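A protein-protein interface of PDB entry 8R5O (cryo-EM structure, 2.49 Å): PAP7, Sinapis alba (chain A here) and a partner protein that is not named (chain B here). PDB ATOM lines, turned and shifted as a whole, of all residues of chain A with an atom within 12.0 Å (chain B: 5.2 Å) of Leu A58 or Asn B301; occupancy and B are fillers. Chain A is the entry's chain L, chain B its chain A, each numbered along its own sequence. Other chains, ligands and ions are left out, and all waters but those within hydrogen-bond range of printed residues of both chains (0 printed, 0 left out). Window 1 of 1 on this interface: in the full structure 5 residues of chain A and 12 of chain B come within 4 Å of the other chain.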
ATOM      1  N   PHE A  56      -2.128  16.250  11.491  1.00  0.00           N
ATOM      2  CA  PHE A  56      -3.459  15.906  11.977  1.00  0.00           C
ATOM      3  C   PHE A  56      -4.216  17.143  12.450  1.00  0.00           C
ATOM      4  O   PHE A  56      -3.606  18.120  12.883  1.00  0.00           O
ATOM      5  CB  PHE A  56      -3.367  14.874  13.104  1.00  0.00           C
ATOM      6  CG  PHE A  56      -3.191  13.466  12.616  1.00  0.00           C
ATOM      7  CD1 PHE A  56      -4.269  12.754  12.121  1.00  0.00           C
ATOM      8  CD2 PHE A  56      -1.949  12.857  12.647  1.00  0.00           C
ATOM      9  CE1 PHE A  56      -4.113  11.462  11.667  1.00  0.00           C
ATOM     10  CE2 PHE A  56      -1.787  11.565  12.195  1.00  0.00           C
ATOM     11  CZ  PHE A  56      -2.869  10.867  11.705  1.00  0.00           C
ATOM     12  N   PRO A  57      -5.548  17.102  12.356  1.00  0.00           N
ATOM     13  CA  PRO A  57      -6.350  18.269  12.765  1.00  0.00           C
ATOM     14  C   PRO A  57      -6.184  18.649  14.224  1.00  0.00           C
ATOM     15  O   PRO A  57      -6.449  19.803  14.582  1.00  0.00           O
ATOM     16  CB  PRO A  57      -7.788  17.826  12.465  1.00  0.00           C
ATOM     17  CG  PRO A  57      -7.648  16.791  11.403  1.00  0.00           C
ATOM     18  CD  PRO A  57      -6.374  16.064  11.718  1.00  0.00           C
ATOM     19  N   LEU A  58      -5.773  17.717  15.084  1.00  0.00           N
ATOM     20  CA  LEU A  58      -5.541  18.038  16.485  1.00  0.00           C
ATOM     21  C   LEU A  58      -4.233  18.787  16.707  1.00  0.00           C
ATOM     22  O   LEU A  58      -4.115  19.521  17.694  1.00  0.00           O
ATOM     23  CB  LEU A  58      -5.558  16.759  17.324  1.00  0.00           C
ATOM     24  CG  LEU A  58      -5.560  16.940  18.842  1.00  0.00           C
ATOM     25  CD1 LEU A  58      -6.649  17.915  19.257  1.00  0.00           C
ATOM     26  CD2 LEU A  58      -5.749  15.604  19.531  1.00  0.00           C
ATOM     27  N   PHE A  59      -3.256  18.630  15.816  1.00  0.00           N
ATOM     28  CA  PHE A  59      -1.946  19.244  15.975  1.00  0.00           C
ATOM     29  C   PHE A  59      -1.787  20.529  15.171  1.00  0.00           C
ATOM     30  O   PHE A  59      -0.677  21.063  15.090  1.00  0.00           O
ATOM     31  CB  PHE A  59      -0.848  18.252  15.591  1.00  0.00           C
ATOM     32  CG  PHE A  59      -0.404  17.372  16.724  1.00  0.00           C
ATOM     33  CD1 PHE A  59       0.501  17.838  17.663  1.00  0.00           C
ATOM     34  CD2 PHE A  59      -0.889  16.082  16.849  1.00  0.00           C
ATOM     35  CE1 PHE A  59       0.913  17.034  18.706  1.00  0.00           C
ATOM     36  CE2 PHE A  59      -0.479  15.274  17.889  1.00  0.00           C
ATOM     37  CZ  PHE A  59       0.421  15.750  18.819  1.00  0.00           C
ATOM     38  N   GLN A  60      -2.860  21.033  14.573  1.00  0.00           N
ATOM     39  CA  GLN A  60      -2.797  22.293  13.846  1.00  0.00           C
ATOM     40  C   GLN A  60      -3.464  23.406  14.646  1.00  0.00           C
ATOM     41  O   GLN A  60      -3.371  23.441  15.872  1.00  0.00           O
ATOM     42  CB  GLN A  60      -3.456  22.162  12.472  1.00  0.00           C
ATOM     43  CG  GLN A  60      -4.887  21.662  12.521  1.00  0.00           C
ATOM     44  CD  GLN A  60      -5.605  21.818  11.198  1.00  0.00           C
ATOM     45  OE1 GLN A  60      -6.296  20.907  10.742  1.00  0.00           O
ATOM     46  NE2 GLN A  60      -5.453  22.981  10.576  1.00  0.00           N
ATOM     47  N   ILE B 292     -15.105   9.152  21.740  1.00  0.00           N
ATOM     48  CA  ILE B 292     -13.775   9.132  21.145  1.00  0.00           C
ATOM     49  C   ILE B 292     -13.024   7.963  21.772  1.00  0.00           C
ATOM     50  O   ILE B 292     -12.669   8.005  22.952  1.00  0.00           O
ATOM     51  CB  ILE B 292     -13.038  10.458  21.364  1.00  0.00           C
ATOM     52  CG1 ILE B 292     -13.785  11.598  20.671  1.00  0.00           C
ATOM     53  CG2 ILE B 292     -11.608  10.363  20.867  1.00  0.00           C
ATOM     54  CD1 ILE B 292     -13.156  12.952  20.876  1.00  0.00           C
ATOM     55  N   ASP B 297      -9.512   8.600  16.169  1.00  0.00           N
ATOM     56  CA  ASP B 297     -10.673   9.426  16.482  1.00  0.00           C
ATOM     57  C   ASP B 297     -10.258  10.701  17.206  1.00  0.00           C
ATOM     58  O   ASP B 297     -10.800  11.779  16.942  1.00  0.00           O
ATOM     59  CB  ASP B 297     -11.673   8.636  17.327  1.00  0.00           C
ATOM     60  CG  ASP B 297     -12.169   7.387  16.629  1.00  0.00           C
ATOM     61  OD1 ASP B 297     -12.210   7.376  15.381  1.00  0.00           O
ATOM     62  OD2 ASP B 297     -12.519   6.414  17.330  1.00  0.00           O
ATOM     63  N   LEU B 298      -9.303  10.591  18.131  1.00  0.00           N
ATOM     64  CA  LEU B 298      -8.816  11.763  18.852  1.00  0.00           C
ATOM     65  C   LEU B 298      -8.117  12.737  17.912  1.00  0.00           C
ATOM     66  O   LEU B 298      -8.289  13.955  18.034  1.00  0.00           O
ATOM     67  CB  LEU B 298      -7.874  11.326  19.974  1.00  0.00           C
ATOM     68  CG  LEU B 298      -7.222  12.399  20.844  1.00  0.00           C
ATOM     69  CD1 LEU B 298      -8.267  13.164  21.637  1.00  0.00           C
ATOM     70  CD2 LEU B 298      -6.196  11.769  21.771  1.00  0.00           C
ATOM     71  N   LEU B 299      -7.324  12.217  16.972  1.00  0.00           N
ATOM     72  CA  LEU B 299      -6.582  13.080  16.056  1.00  0.00           C
ATOM     73  C   LEU B 299      -7.516  13.894  15.168  1.00  0.00           C
ATOM     74  O   LEU B 299      -7.298  15.094  14.963  1.00  0.00           O
ATOM     75  CB  LEU B 299      -5.634  12.239  15.205  1.00  0.00           C
ATOM     76  CG  LEU B 299      -4.502  11.529  15.951  1.00  0.00           C
ATOM     77  CD1 LEU B 299      -3.753  10.595  15.020  1.00  0.00           C
ATOM     78  CD2 LEU B 299      -3.556  12.541  16.573  1.00  0.00           C
ATOM     79  N   ASN B 300      -8.563  13.263  14.630  1.00  0.00           N
ATOM     80  CA  ASN B 300      -9.472  13.966  13.731  1.00  0.00           C
ATOM     81  C   ASN B 300     -10.248  15.075  14.430  1.00  0.00           C
ATOM     82  O   ASN B 300     -10.740  15.985  13.755  1.00  0.00           O
ATOM     83  CB  ASN B 300     -10.441  12.978  13.083  1.00  0.00           C
ATOM     84  CG  ASN B 300      -9.802  12.197  11.954  1.00  0.00           C
ATOM     85  OD1 ASN B 300      -8.579  12.160  11.826  1.00  0.00           O
ATOM     86  ND2 ASN B 300     -10.628  11.572  11.125  1.00  0.00           N
ATOM     87  N   ASN B 301     -10.372  15.023  15.752  1.00  0.00           N
ATOM     88  CA  ASN B 301     -10.969  16.131  16.483  1.00  0.00           C
ATOM     89  C   ASN B 301     -10.004  17.306  16.527  1.00  0.00           C
ATOM     90  O   ASN B 301      -8.805  17.138  16.770  1.00  0.00           O
ATOM     91  CB  ASN B 301     -11.339  15.701  17.902  1.00  0.00           C
ATOM     92  CG  ASN B 301     -12.708  15.060  17.978  1.00  0.00           C
ATOM     93  OD1 ASN B 301     -12.871  13.877  17.681  1.00  0.00           O
ATOM     94  ND2 ASN B 301     -13.702  15.839  18.388  1.00  0.00           N
ATOM     95  N   SER B 302     -10.529  18.504  16.291  1.00  0.00           N
ATOM     96  CA  SER B 302      -9.709  19.707  16.303  1.00  0.00           C
ATOM     97  C   SER B 302      -9.477  20.143  17.746  1.00  0.00           C
ATOM     98  O   SER B 302      -9.798  19.429  18.699  1.00  0.00           O
ATOM     99  CB  SER B 302     -10.365  20.805  15.470  1.00  0.00           C
ATOM    100  OG  SER B 302     -11.459  21.382  16.161  1.00  0.00           O
ATOM    101  N   GLN B 303      -8.908  21.333  17.927  1.00  0.00           N
ATOM    102  CA  GLN B 303      -8.702  21.876  19.261  1.00  0.00           C
ATOM    103  C   GLN B 303      -9.876  22.715  19.741  1.00  0.00           C
ATOM    104  O   GLN B 303     -10.017  22.921  20.952  1.00  0.00           O
ATOM    105  CB  GLN B 303      -7.422  22.714  19.301  1.00  0.00           C
ATOM    106  CG  GLN B 303      -6.176  21.944  18.904  1.00  0.00           C
ATOM    107  CD  GLN B 303      -4.914  22.772  19.025  1.00  0.00           C
ATOM    108  OE1 GLN B 303      -3.881  22.436  18.446  1.00  0.00           O
ATOM    109  NE2 GLN B 303      -4.988  23.858  19.785  1.00  0.00           N
ATOM    110  N   ASP B 305     -13.074  21.740  18.996  1.00  0.00           N
ATOM    111  CA  ASP B 305     -14.089  20.743  19.324  1.00  0.00           C
ATOM    112  C   ASP B 305     -13.925  20.235  20.751  1.00  0.00           C
ATOM    113  O   ASP B 305     -14.907  20.086  21.485  1.00  0.00           O
ATOM    114  CB  ASP B 305     -14.020  19.582  18.332  1.00  0.00           C
ATOM    115  CG  ASP B 305     -14.086  20.040  16.890  1.00  0.00           C
ATOM    116  OD1 ASP B 305     -14.792  21.030  16.610  1.00  0.00           O
ATOM    117  OD2 ASP B 305     -13.428  19.410  16.035  1.00  0.00           O
ATOM    118  N   LEU B 306     -12.683  19.962  21.160  1.00  0.00           N
ATOM    119  CA  LEU B 306     -12.446  19.439  22.501  1.00  0.00           C
ATOM    120  C   LEU B 306     -12.849  20.441  23.576  1.00  0.00           C
ATOM    121  O   LEU B 306     -13.301  20.042  24.655  1.00  0.00           O
ATOM    122  CB  LEU B 306     -10.977  19.049  22.660  1.00  0.00           C
ATOM    123  CG  LEU B 306     -10.424  18.014  21.678  1.00  0.00           C
ATOM    124  CD1 LEU B 306      -8.980  17.684  22.010  1.00  0.00           C
ATOM    125  CD2 LEU B 306     -11.277  16.755  21.673  1.00  0.00           C
ATOM    126  N   LEU B 320      -2.699  17.521  27.098  1.00  0.00           N
ATOM    127  CA  LEU B 320      -3.093  16.450  26.188  1.00  0.00           C
ATOM    128  C   LEU B 320      -2.216  16.437  24.942  1.00  0.00           C
ATOM    129  O   LEU B 320      -1.806  15.368  24.475  1.00  0.00           O
ATOM    130  CB  LEU B 320      -4.564  16.596  25.805  1.00  0.00           C
ATOM    131  CG  LEU B 320      -5.057  15.737  24.637  1.00  0.00           C
ATOM    132  CD1 LEU B 320      -4.963  14.254  24.964  1.00  0.00           C
ATOM    133  CD2 LEU B 320      -6.476  16.116  24.253  1.00  0.00           C
ATOM    134  N   LEU B 321      -1.918  17.617  24.388  1.00  0.00           N
ATOM    135  CA  LEU B 321      -1.042  17.684  23.223  1.00  0.00           C
ATOM    136  C   LEU B 321       0.361  17.198  23.557  1.00  0.00           C
ATOM    137  O   LEU B 321       1.002  16.526  22.743  1.00  0.00           O
ATOM    138  CB  LEU B 321      -0.999  19.111  22.675  1.00  0.00           C
ATOM    139  CG  LEU B 321      -2.247  19.612  21.944  1.00  0.00           C
ATOM    140  CD1 LEU B 321      -1.995  20.982  21.333  1.00  0.00           C
ATOM    141  CD2 LEU B 321      -2.683  18.618  20.881  1.00  0.00           C
ATOM    142  N   LEU B 324       0.494  13.559  23.449  1.00  0.00           N
ATOM    143  CA  LEU B 324       0.536  13.186  22.040  1.00  0.00           C
ATOM    144  C   LEU B 324       1.806  13.678  21.359  1.00  0.00           C
ATOM    145  O   LEU B 324       2.275  13.046  20.406  1.00  0.00           O
ATOM    146  CB  LEU B 324      -0.698  13.731  21.321  1.00  0.00           C
ATOM    147  CG  LEU B 324      -2.033  13.210  21.850  1.00  0.00           C
ATOM    148  CD1 LEU B 324      -3.191  13.891  21.151  1.00  0.00           C
ATOM    149  CD2 LEU B 324      -2.114  11.704  21.681  1.00  0.00           C
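O of Leu B299 is in hydrogen-bond range of N of Leu A58 (3.0 Å).
OE1 of Gln B303 sits close to O of Leu A58 (3.0 Å).
The backbone carbonyl oxygen (O) of Gln A60 sits close to the side-chain amide oxygen (OE1) of Gln B303 (2.8 Å).
The side-chain amide oxygen (OD1) of Asn B301 lies close to the backbone carbonyl oxygen (O) of Asp B297 (3.0 Å).
The side-chain carboxylate of Asp B305 lies within hydrogen-bond range of the side-chain hydroxyl of Ser B302 (2.8 Å).
Among the printed residues, merely in contact across the chains: Leu A58 with Asn B301 (3.3 Å), Leu A58 with Leu B298 (3.4 Å), Phe A59 with Leu B324 (3.4 Å), Phe A56 with Leu B299 (3.4 Å), Leu A58 with Leu B324 (3.5 Å), Pro A57 with Leu B299 (3.5 Å), Leu A58 with Ser B302 (3.5 Å), Leu A58 with Leu B321 (3.6 Å), Leu A58 with Leu B306 (3.6 Å), Pro A57 with Ser B302 (3.7 Å), Pro A57 with Asn B300 (3.7 Å) and Pro A57 with Asn B301 (3.95 Å).
Printed residues of chain B within 4 Å of Phe A56: Leu B299 (3.4 Å).
Printed residues of chain B within 4 Å of Pro A57: Leu B299, Asn B300, Asn B301 and Ser B302.
Leu A58 touches just these residues of chain B: Leu B298, Leu B299, Asn B301, Ser B302, Gln B303, Leu B306, Leu B321 and Leu B324.
Printed residues of chain B within 4 Å of Phe A59: Leu B324.
Printed residues of chain B within 4 Å of Gln A60: Gln B303.
Leu B298 touches just one residue of chain A: Leu A58.
Leu B299 touches just these residues of chain A: Phe A56 (3.4 Å), Pro A57 (3.5 Å) and Leu A58 (3.0 Å).
Asn B300 touches one residue of chain A.
Of chain A, only Pro A57 (3.95 Å) and Leu A58 (3.3 Å) come within 4 Å of Asn B301.
Ser B302 touches just these residues of chain A: Pro A57 (3.7 Å) and Leu A58 (3.5 Å).
No residue of chain A comes within 4 Å of Asp B305.
Of chain A, only Leu A58 comes within 4 Å of Leu B306.
Leu B320 touches none of the printed residues of chain A.
Leu B321 touches just one residue of chain A: Leu A58.
Printed residues of chain A within 4 Å of Leu B324: Leu A58 and Phe A59.
Of the 13 printed residues of chain B, 9 touch a printed residue of chain A.
Hydrophobic or aromatic side chains of chain B within 4 Å of the printed part of chain A: Leu B298, Leu B299, Leu B306, Leu B321 and Leu B324.
Hydrophobic or aromatic side chains of chain A that line the printed part of chain B: Phe A56, Pro A57, Leu A58 and Phe A59.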
